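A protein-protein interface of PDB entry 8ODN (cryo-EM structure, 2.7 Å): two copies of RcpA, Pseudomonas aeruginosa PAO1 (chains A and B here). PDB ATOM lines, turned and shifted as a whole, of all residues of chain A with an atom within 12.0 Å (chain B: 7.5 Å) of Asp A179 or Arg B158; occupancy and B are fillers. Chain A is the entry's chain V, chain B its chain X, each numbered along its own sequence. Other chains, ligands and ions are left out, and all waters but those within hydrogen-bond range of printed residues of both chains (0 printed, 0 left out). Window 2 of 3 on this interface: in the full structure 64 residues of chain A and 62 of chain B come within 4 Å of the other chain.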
ATOM      1  N   ARG A 158      -8.564  34.718  32.671  1.00  0.00           N
ATOM      2  CA  ARG A 158      -7.224  35.208  32.957  1.00  0.00           C
ATOM      3  C   ARG A 158      -7.066  35.425  34.456  1.00  0.00           C
ATOM      4  O   ARG A 158      -8.035  35.402  35.219  1.00  0.00           O
ATOM      5  CB  ARG A 158      -6.939  36.513  32.199  1.00  0.00           C
ATOM      6  CG  ARG A 158      -7.109  36.412  30.689  1.00  0.00           C
ATOM      7  CD  ARG A 158      -6.034  35.550  30.055  1.00  0.00           C
ATOM      8  NE  ARG A 158      -4.714  36.164  30.147  1.00  0.00           N
ATOM      9  CZ  ARG A 158      -4.245  37.068  29.298  1.00  0.00           C
ATOM     10  NH1 ARG A 158      -4.972  37.512  28.286  1.00  0.00           N
ATOM     11  NH2 ARG A 158      -3.015  37.543  29.470  1.00  0.00           N
ATOM     12  N   GLY A 160      -3.645  34.666  37.165  1.00  0.00           N
ATOM     13  CA  GLY A 160      -3.037  33.543  37.849  1.00  0.00           C
ATOM     14  C   GLY A 160      -3.188  32.278  37.034  1.00  0.00           C
ATOM     15  O   GLY A 160      -2.218  31.745  36.487  1.00  0.00           O
ATOM     16  N   ASN A 161      -4.422  31.793  36.956  1.00  0.00           N
ATOM     17  CA  ASN A 161      -4.780  30.693  36.080  1.00  0.00           C
ATOM     18  C   ASN A 161      -5.087  31.215  34.679  1.00  0.00           C
ATOM     19  O   ASN A 161      -5.175  32.421  34.436  1.00  0.00           O
ATOM     20  CB  ASN A 161      -5.983  29.940  36.640  1.00  0.00           C
ATOM     21  CG  ASN A 161      -5.736  29.401  38.033  1.00  0.00           C
ATOM     22  OD1 ASN A 161      -4.636  28.946  38.348  1.00  0.00           O
ATOM     23  ND2 ASN A 161      -6.757  29.456  38.879  1.00  0.00           N
ATOM     24  N   LEU A 162      -5.245  30.281  33.746  1.00  0.00           N
ATOM     25  CA  LEU A 162      -5.669  30.609  32.393  1.00  0.00           C
ATOM     26  C   LEU A 162      -6.496  29.451  31.865  1.00  0.00           C
ATOM     27  O   LEU A 162      -6.085  28.295  31.977  1.00  0.00           O
ATOM     28  CB  LEU A 162      -4.468  30.876  31.480  1.00  0.00           C
ATOM     29  CG  LEU A 162      -4.808  31.306  30.053  1.00  0.00           C
ATOM     30  CD1 LEU A 162      -3.827  32.361  29.571  1.00  0.00           C
ATOM     31  CD2 LEU A 162      -4.805  30.115  29.114  1.00  0.00           C
ATOM     32  N   LYS A 175      -2.090  31.706  18.546  1.00  0.00           N
ATOM     33  CA  LYS A 175      -1.035  30.853  19.065  1.00  0.00           C
ATOM     34  C   LYS A 175      -0.604  31.383  20.425  1.00  0.00           C
ATOM     35  O   LYS A 175      -0.621  32.593  20.668  1.00  0.00           O
ATOM     36  CB  LYS A 175       0.171  30.809  18.117  1.00  0.00           C
ATOM     37  CG  LYS A 175      -0.177  30.490  16.670  1.00  0.00           C
ATOM     38  CD  LYS A 175      -0.738  29.085  16.521  1.00  0.00           C
ATOM     39  CE  LYS A 175      -1.163  28.801  15.088  1.00  0.00           C
ATOM     40  NZ  LYS A 175      -0.013  28.816  14.141  1.00  0.00           N
ATOM     41  N   VAL A 176      -0.216  30.473  21.314  1.00  0.00           N
ATOM     42  CA  VAL A 176       0.199  30.817  22.668  1.00  0.00           C
ATOM     43  C   VAL A 176       1.718  30.750  22.740  1.00  0.00           C
ATOM     44  O   VAL A 176       2.344  29.902  22.092  1.00  0.00           O
ATOM     45  CB  VAL A 176      -0.447  29.893  23.719  1.00  0.00           C
ATOM     46  CG1 VAL A 176      -0.098  28.440  23.450  1.00  0.00           C
ATOM     47  CG2 VAL A 176      -0.013  30.300  25.120  1.00  0.00           C
ATOM     48  N   ASN A 177       2.307  31.645  23.529  1.00  0.00           N
ATOM     49  CA  ASN A 177       3.753  31.776  23.562  1.00  0.00           C
ATOM     50  C   ASN A 177       4.389  30.584  24.276  1.00  0.00           C
ATOM     51  O   ASN A 177       3.719  29.766  24.914  1.00  0.00           O
ATOM     52  CB  ASN A 177       4.159  33.082  24.246  1.00  0.00           C
ATOM     53  CG  ASN A 177       3.921  33.058  25.743  1.00  0.00           C
ATOM     54  OD1 ASN A 177       4.654  32.408  26.489  1.00  0.00           O
ATOM     55  ND2 ASN A 177       2.901  33.779  26.192  1.00  0.00           N
ATOM     56  N   ALA A 178       5.716  30.496  24.154  1.00  0.00           N
ATOM     57  CA  ALA A 178       6.445  29.363  24.713  1.00  0.00           C
ATOM     58  C   ALA A 178       6.348  29.312  26.230  1.00  0.00           C
ATOM     59  O   ALA A 178       6.244  28.224  26.807  1.00  0.00           O
ATOM     60  CB  ALA A 178       7.913  29.428  24.289  1.00  0.00           C
ATOM     61  N   ASP A 179       6.375  30.465  26.894  1.00  0.00           N
ATOM     62  CA  ASP A 179       6.424  30.513  28.349  1.00  0.00           C
ATOM     63  C   ASP A 179       5.042  30.492  28.990  1.00  0.00           C
ATOM     64  O   ASP A 179       4.945  30.530  30.221  1.00  0.00           O
ATOM     65  CB  ASP A 179       7.184  31.763  28.804  1.00  0.00           C
ATOM     66  CG  ASP A 179       7.709  31.644  30.223  1.00  0.00           C
ATOM     67  OD1 ASP A 179       7.462  30.604  30.869  1.00  0.00           O
ATOM     68  OD2 ASP A 179       8.377  32.590  30.692  1.00  0.00           O
ATOM     69  N   GLY A 180       3.977  30.430  28.195  1.00  0.00           N
ATOM     70  CA  GLY A 180       2.645  30.291  28.749  1.00  0.00           C
ATOM     71  C   GLY A 180       2.150  31.485  29.530  1.00  0.00           C
ATOM     72  O   GLY A 180       1.251  31.336  30.361  1.00  0.00           O
ATOM     73  N   SER A 181       2.711  32.670  29.291  1.00  0.00           N
ATOM     74  CA  SER A 181       2.285  33.862  30.015  1.00  0.00           C
ATOM     75  C   SER A 181       1.005  34.468  29.456  1.00  0.00           C
ATOM     76  O   SER A 181       0.375  35.284  30.137  1.00  0.00           O
ATOM     77  CB  SER A 181       3.399  34.911  29.995  1.00  0.00           C
ATOM     78  OG  SER A 181       3.740  35.267  28.667  1.00  0.00           O
ATOM     79  N   GLY A 182       0.611  34.094  28.246  1.00  0.00           N
ATOM     80  CA  GLY A 182      -0.589  34.647  27.647  1.00  0.00           C
ATOM     81  C   GLY A 182      -0.666  34.298  26.180  1.00  0.00           C
ATOM     82  O   GLY A 182       0.297  33.827  25.572  1.00  0.00           O
ATOM     83  N   LEU A 183      -1.846  34.539  25.614  1.00  0.00           N
ATOM     84  CA  LEU A 183      -2.067  34.279  24.201  1.00  0.00           C
ATOM     85  C   LEU A 183      -1.351  35.318  23.345  1.00  0.00           C
ATOM     86  O   LEU A 183      -1.090  36.442  23.780  1.00  0.00           O
ATOM     87  CB  LEU A 183      -3.564  34.283  23.885  1.00  0.00           C
ATOM     88  CG  LEU A 183      -4.413  33.303  24.692  1.00  0.00           C
ATOM     89  CD1 LEU A 183      -5.884  33.475  24.353  1.00  0.00           C
ATOM     90  CD2 LEU A 183      -3.968  31.876  24.438  1.00  0.00           C
ATOM     91  N   GLY A 184      -1.032  34.926  22.114  1.00  0.00           N
ATOM     92  CA  GLY A 184      -0.287  35.781  21.211  1.00  0.00           C
ATOM     93  C   GLY A 184      -0.962  36.014  19.873  1.00  0.00           C
ATOM     94  O   GLY A 184      -0.279  36.195  18.861  1.00  0.00           O
ATOM     95  N   VAL B 156       3.339  20.788  29.288  1.00  0.00           N
ATOM     96  CA  VAL B 156       4.693  21.277  29.499  1.00  0.00           C
ATOM     97  C   VAL B 156       4.839  21.668  30.963  1.00  0.00           C
ATOM     98  O   VAL B 156       3.868  22.036  31.628  1.00  0.00           O
ATOM     99  CB  VAL B 156       5.024  22.480  28.587  1.00  0.00           C
ATOM    100  CG1 VAL B 156       6.407  23.038  28.903  1.00  0.00           C
ATOM    101  CG2 VAL B 156       4.927  22.080  27.128  1.00  0.00           C
ATOM    102  N   ARG B 157       6.070  21.588  31.462  1.00  0.00           N
ATOM    103  CA  ARG B 157       6.374  21.983  32.829  1.00  0.00           C
ATOM    104  C   ARG B 157       7.688  22.751  32.838  1.00  0.00           C
ATOM    105  O   ARG B 157       8.528  22.594  31.949  1.00  0.00           O
ATOM    106  CB  ARG B 157       6.450  20.768  33.762  1.00  0.00           C
ATOM    107  CG  ARG B 157       6.366  21.123  35.235  1.00  0.00           C
ATOM    108  CD  ARG B 157       6.290  19.887  36.111  1.00  0.00           C
ATOM    109  NE  ARG B 157       5.990  20.230  37.497  1.00  0.00           N
ATOM    110  CZ  ARG B 157       6.884  20.676  38.370  1.00  0.00           C
ATOM    111  NH1 ARG B 157       8.154  20.843  38.037  1.00  0.00           N
ATOM    112  NH2 ARG B 157       6.493  20.964  39.608  1.00  0.00           N
ATOM    113  N   ARG B 158       7.858  23.586  33.861  1.00  0.00           N
ATOM    114  CA  ARG B 158       8.977  24.516  33.923  1.00  0.00           C
ATOM    115  C   ARG B 158       9.473  24.625  35.360  1.00  0.00           C
ATOM    116  O   ARG B 158       8.829  24.162  36.305  1.00  0.00           O
ATOM    117  CB  ARG B 158       8.576  25.899  33.393  1.00  0.00           C
ATOM    118  CG  ARG B 158       8.026  25.894  31.973  1.00  0.00           C
ATOM    119  CD  ARG B 158       9.101  25.570  30.952  1.00  0.00           C
ATOM    120  NE  ARG B 158      10.104  26.623  30.859  1.00  0.00           N
ATOM    121  CZ  ARG B 158       9.978  27.718  30.121  1.00  0.00           C
ATOM    122  NH1 ARG B 158       8.887  27.952  29.408  1.00  0.00           N
ATOM    123  NH2 ARG B 158      10.971  28.603  30.097  1.00  0.00           N
ATOM    124  N   GLY B 159      10.643  25.243  35.511  1.00  0.00           N
ATOM    125  CA  GLY B 159      11.219  25.510  36.815  1.00  0.00           C
ATOM    126  C   GLY B 159      12.318  24.537  37.181  1.00  0.00           C
ATOM    127  O   GLY B 159      12.041  23.418  37.623  1.00  0.00           O
ATOM    128  N   GLY B 160      13.570  24.950  37.010  1.00  0.00           N
ATOM    129  CA  GLY B 160      14.690  24.079  37.301  1.00  0.00           C
ATOM    130  C   GLY B 160      14.750  22.938  36.310  1.00  0.00           C
ATOM    131  O   GLY B 160      15.644  22.868  35.461  1.00  0.00           O
ATOM    132  N   ASN B 161      13.783  22.032  36.422  1.00  0.00           N
ATOM    133  CA  ASN B 161      13.584  20.973  35.452  1.00  0.00           C
ATOM    134  C   ASN B 161      12.733  21.477  34.290  1.00  0.00           C
ATOM    135  O   ASN B 161      12.177  22.577  34.316  1.00  0.00           O
ATOM    136  CB  ASN B 161      12.917  19.769  36.113  1.00  0.00           C
ATOM    137  CG  ASN B 161      13.719  19.228  37.278  1.00  0.00           C
ATOM    138  OD1 ASN B 161      14.949  19.193  37.236  1.00  0.00           O
ATOM    139  ND2 ASN B 161      13.026  18.809  38.330  1.00  0.00           N
ATOM    140  N   LEU B 162      12.640  20.650  33.253  1.00  0.00           N
ATOM    141  CA  LEU B 162      11.764  20.926  32.125  1.00  0.00           C
ATOM    142  C   LEU B 162      11.260  19.600  31.582  1.00  0.00           C
ATOM    143  O   LEU B 162      12.052  18.680  31.368  1.00  0.00           O
ATOM    144  CB  LEU B 162      12.491  21.716  31.032  1.00  0.00           C
ATOM    145  CG  LEU B 162      11.633  22.126  29.833  1.00  0.00           C
ATOM    146  CD1 LEU B 162      12.019  23.515  29.357  1.00  0.00           C
ATOM    147  CD2 LEU B 162      11.770  21.123  28.703  1.00  0.00           C
ATOM    148  N   TRP B 163       9.952  19.502  31.377  1.00  0.00           N
ATOM    149  CA  TRP B 163       9.335  18.310  30.822  1.00  0.00           C
ATOM    150  C   TRP B 163       8.401  18.703  29.689  1.00  0.00           C
ATOM    151  O   TRP B 163       7.788  19.772  29.709  1.00  0.00           O
ATOM    152  CB  TRP B 163       8.553  17.524  31.880  1.00  0.00           C
ATOM    153  CG  TRP B 163       9.408  16.902  32.937  1.00  0.00           C
ATOM    154  CD1 TRP B 163       9.776  17.459  34.126  1.00  0.00           C
ATOM    155  CD2 TRP B 163       9.996  15.596  32.907  1.00  0.00           C
ATOM    156  NE1 TRP B 163      10.559  16.583  34.837  1.00  0.00           N
ATOM    157  CE2 TRP B 163      10.709  15.432  34.110  1.00  0.00           C
ATOM    158  CE3 TRP B 163       9.990  14.551  31.979  1.00  0.00           C
ATOM    159  CZ2 TRP B 163      11.409  14.265  34.408  1.00  0.00           C
ATOM    160  CZ3 TRP B 163      10.686  13.395  32.277  1.00  0.00           C
ATOM    161  CH2 TRP B 163      11.385  13.261  33.481  1.00  0.00           C
ATOM    162  N   VAL B 164       8.302  17.823  28.698  1.00  0.00           N
ATOM    163  CA  VAL B 164       7.410  18.025  27.565  1.00  0.00           C
ATOM    164  C   VAL B 164       6.901  16.667  27.113  1.00  0.00           C
ATOM    165  O   VAL B 164       7.646  15.684  27.097  1.00  0.00           O
ATOM    166  CB  VAL B 164       8.114  18.760  26.404  1.00  0.00           C
ATOM    167  CG1 VAL B 164       7.149  18.965  25.252  1.00  0.00           C
ATOM    168  CG2 VAL B 164       8.688  20.087  26.874  1.00  0.00           C
ATOM    169  N   SER B 181      17.701  26.299  27.655  1.00  0.00           N
ATOM    170  CA  SER B 181      17.123  27.163  28.678  1.00  0.00           C
ATOM    171  C   SER B 181      15.610  27.293  28.557  1.00  0.00           C
ATOM    172  O   SER B 181      14.964  27.737  29.511  1.00  0.00           O
ATOM    173  CB  SER B 181      17.763  28.551  28.610  1.00  0.00           C
ATOM    174  OG  SER B 181      17.569  29.141  27.337  1.00  0.00           O
ATOM    175  N   GLY B 182      15.038  26.921  27.420  1.00  0.00           N
ATOM    176  CA  GLY B 182      13.605  27.034  27.233  1.00  0.00           C
ATOM    177  C   GLY B 182      13.234  26.830  25.783  1.00  0.00           C
ATOM    178  O   GLY B 182      14.085  26.820  24.890  1.00  0.00           O
ATOM    179  N   LEU B 183      11.933  26.664  25.562  1.00  0.00           N
ATOM    180  CA  LEU B 183      11.420  26.480  24.214  1.00  0.00           C
ATOM    181  C   LEU B 183      11.467  27.793  23.439  1.00  0.00           C
ATOM    182  O   LEU B 183      11.445  28.883  24.015  1.00  0.00           O
ATOM    183  CB  LEU B 183       9.986  25.950  24.256  1.00  0.00           C
ATOM    184  CG  LEU B 183       9.784  24.647  25.026  1.00  0.00           C
ATOM    185  CD1 LEU B 183       8.310  24.284  25.074  1.00  0.00           C
ATOM    186  CD2 LEU B 183      10.594  23.527  24.400  1.00  0.00           C
ATOM    187  N   GLY B 185       9.388  28.417  20.456  1.00  0.00           N
ATOM    188  CA  GLY B 185       8.311  28.465  19.491  1.00  0.00           C
ATOM    189  C   GLY B 185       6.971  28.669  20.170  1.00  0.00           C
ATOM    190  O   GLY B 185       6.858  28.628  21.396  1.00  0.00           O
ATOM    191  N   THR B 186       5.953  28.887  19.342  1.00  0.00           N
ATOM    192  CA  THR B 186       4.592  29.128  19.802  1.00  0.00           C
ATOM    193  C   THR B 186       3.732  27.905  19.510  1.00  0.00           C
ATOM    194  O   THR B 186       3.775  27.359  18.402  1.00  0.00           O
ATOM    195  CB  THR B 186       3.995  30.364  19.126  1.00  0.00           C
ATOM    196  OG1 THR B 186       4.041  30.209  17.702  1.00  0.00           O
ATOM    197  CG2 THR B 186       4.766  31.616  19.522  1.00  0.00           C
ATOM    198  N   PHE B 187       2.957  27.482  20.505  1.00  0.00           N
ATOM    199  CA  PHE B 187       2.092  26.321  20.346  1.00  0.00           C
ATOM    200  C   PHE B 187       0.909  26.638  19.441  1.00  0.00           C
ATOM    201  O   PHE B 187       0.400  27.762  19.425  1.00  0.00           O
ATOM    202  CB  PHE B 187       1.586  25.844  21.708  1.00  0.00           C
ATOM    203  CG  PHE B 187       2.416  24.756  22.319  1.00  0.00           C
ATOM    204  CD1 PHE B 187       2.299  23.451  21.873  1.00  0.00           C
ATOM    205  CD2 PHE B 187       3.308  25.033  23.340  1.00  0.00           C
ATOM    206  CE1 PHE B 187       3.059  22.443  22.430  1.00  0.00           C
ATOM    207  CE2 PHE B 187       4.072  24.029  23.902  1.00  0.00           C
ATOM    208  CZ  PHE B 187       3.946  22.731  23.446  1.00  0.00           C
ATOM    209  N   GLY B 201       0.851  28.549  35.624  1.00  0.00           N
ATOM    210  CA  GLY B 201       2.160  28.954  36.092  1.00  0.00           C
ATOM    211  C   GLY B 201       3.247  28.098  35.479  1.00  0.00           C
ATOM    212  O   GLY B 201       3.584  28.258  34.303  1.00  0.00           O
ATOM    213  N   LYS B 202       3.810  27.185  36.271  1.00  0.00           N
ATOM    214  CA  LYS B 202       4.771  26.233  35.724  1.00  0.00           C
ATOM    215  C   LYS B 202       4.098  25.279  34.746  1.00  0.00           C
ATOM    216  O   LYS B 202       4.600  25.049  33.640  1.00  0.00           O
ATOM    217  CB  LYS B 202       5.446  25.463  36.860  1.00  0.00           C
ATOM    218  CG  LYS B 202       6.331  26.327  37.747  1.00  0.00           C
ATOM    219  CD  LYS B 202       6.855  25.551  38.946  1.00  0.00           C
ATOM    220  CE  LYS B 202       7.749  26.417  39.822  1.00  0.00           C
ATOM    221  NZ  LYS B 202       8.188  25.702  41.051  1.00  0.00           N
ATOM    222  N   TRP B 203       2.956  24.715  35.134  1.00  0.00           N
ATOM    223  CA  TRP B 203       2.246  23.785  34.270  1.00  0.00           C
ATOM    224  C   TRP B 203       1.617  24.505  33.082  1.00  0.00           C
ATOM    225  O   TRP B 203       1.190  25.659  33.176  1.00  0.00           O
ATOM    226  CB  TRP B 203       1.159  23.049  35.053  1.00  0.00           C
ATOM    227  CG  TRP B 203       1.677  21.984  35.970  1.00  0.00           C
ATOM    228  CD1 TRP B 203       1.968  22.114  37.296  1.00  0.00           C
ATOM    229  CD2 TRP B 203       1.957  20.621  35.629  1.00  0.00           C
ATOM    230  NE1 TRP B 203       2.414  20.916  37.802  1.00  0.00           N
ATOM    231  CE2 TRP B 203       2.417  19.985  36.798  1.00  0.00           C
ATOM    232  CE3 TRP B 203       1.865  19.878  34.449  1.00  0.00           C
ATOM    233  CZ2 TRP B 203       2.784  18.641  36.821  1.00  0.00           C
ATOM    234  CZ3 TRP B 203       2.230  18.545  34.474  1.00  0.00           C
ATOM    235  CH2 TRP B 203       2.684  17.941  35.651  1.00  0.00           C
ATOM    236  N   LEU B 204       1.564  23.801  31.953  1.00  0.00           N
ATOM    237  CA  LEU B 204       0.851  24.262  30.770  1.00  0.00           C
ATOM    238  C   LEU B 204       0.400  23.033  29.999  1.00  0.00           C
ATOM    239  O   LEU B 204       1.215  22.153  29.712  1.00  0.00           O
ATOM    240  CB  LEU B 204       1.732  25.162  29.896  1.00  0.00           C
ATOM    241  CG  LEU B 204       1.133  25.603  28.556  1.00  0.00           C
ATOM    242  CD1 LEU B 204      -0.179  26.339  28.764  1.00  0.00           C
ATOM    243  CD2 LEU B 204       2.116  26.476  27.791  1.00  0.00           C
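N of Gly A184 is in hydrogen-bond range of O of Lys A175, at 2.8 Å.
OD1 of Asn A177 lies within hydrogen-bond range of N of Asp A179 (2.6 Å).
The backbone NH of Gly A180 lies within hydrogen-bond range of the side-chain amide oxygen of Asn A177.
The backbone carbonyl oxygen (O) of Leu B204 is in hydrogen-bond range of the backbone NH (N) of Val B156, at 2.6 Å.
Asp A179 touches one residue of chain B.
Of the printed residues of chain B, Ala A178 touches Arg B158, Leu B183 and Gly B185.
No residue of chain A comes within 4 Å of Val B156.
No residue of chain A comes within 4 Å of Arg B157.
No residue of chain A comes within 4 Å of Gly B159.
No residue of chain A comes within 4 Å of Asn B161.
No residue of chain A comes within 4 Å of Leu B162.
No residue of chain A comes within 4 Å of Gly B182.
Leu B183 touches just one residue of chain A: Ala A178 (3.6 Å).
Of chain A, only Ala A178 (3.2 Å) comes within 4 Å of Gly B185.
No residue of chain A comes within 4 Å of Gly B201.
No residue of chain A comes within 4 Å of Trp B203.
Of the printed residues of chain A, Leu B204 touches Gly A180 (3.97 Å).
Printed residues of chain A within 4 Å of Phe B187: Lys A175 and Val A176.
Of the printed residues of chain B, Val A176 touches Thr B186 and Phe B187.
Of the printed residues of chain B, Lys A175 touches Thr B186 and Phe B187.
Gly A160 touches none of the printed residues of chain B.
Arg A158 touches none of the printed residues of chain B.
The nearest residue of chain B that does not touch Asp A179 is Gly B201 (4.9 Å).
The nearest residue of chain A that does not touch Arg B158 is Gly A180 (5.6 Å).
Positions printed for both chains: 158, 160, 161, 162, 181, 182 and 183.
Of the 9 pairs that touch across the chains among the printed residues, none has its exchanged pair printed and touching as well.
Thr B186 touches Lys A175 (OG1 to CB, 3.9 Å).
O of Phe B187 touches CB of Lys A175, at 3.3 Å.
Thr B186 touches Val A176 (CA to O, 3.3 Å).
Arg B158 touches Ala A178 (NH1 to O, 3.7 Å).
Ala A178 touches Leu B183.
O of Gly B185 touches CB of Ala A178, at 3.2 Å.
CD2 of Leu B204 touches CA of Gly A180 (3.97 Å).
Hydrophobic or aromatic side chains of chain A that line the printed part of chain B: Val A176 and Ala A178.
Of the 19 printed residues of chain B, 6 touch a printed residue of chain A.
Printed residues of chain B that touch a printed residue of chain A: Arg B158, Leu B183, Gly B185, Thr B186, Phe B187 and Leu B204.
Along chain B the printed residues that touch a printed residue of chain A span positions 158 to 204.
Among the printed residues, 9 pairs touch across the chains.
Among the printed residues, Asp or Glu carboxylates within 4 Å of a Lys or Arg side-chain nitrogen of the other chain: Asp A179 with Arg B158 (3.3 Å).
The backbone NH of Phe B187 sits at hydrogen-bond distance from the backbone carbonyl oxygen of Val A176, at 3.0 Å.
The guanidinium group (NH1) of Arg B158 is in salt-bridge range of the side-chain carboxylate (OD1) of Asp A179 (3.3 Å).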
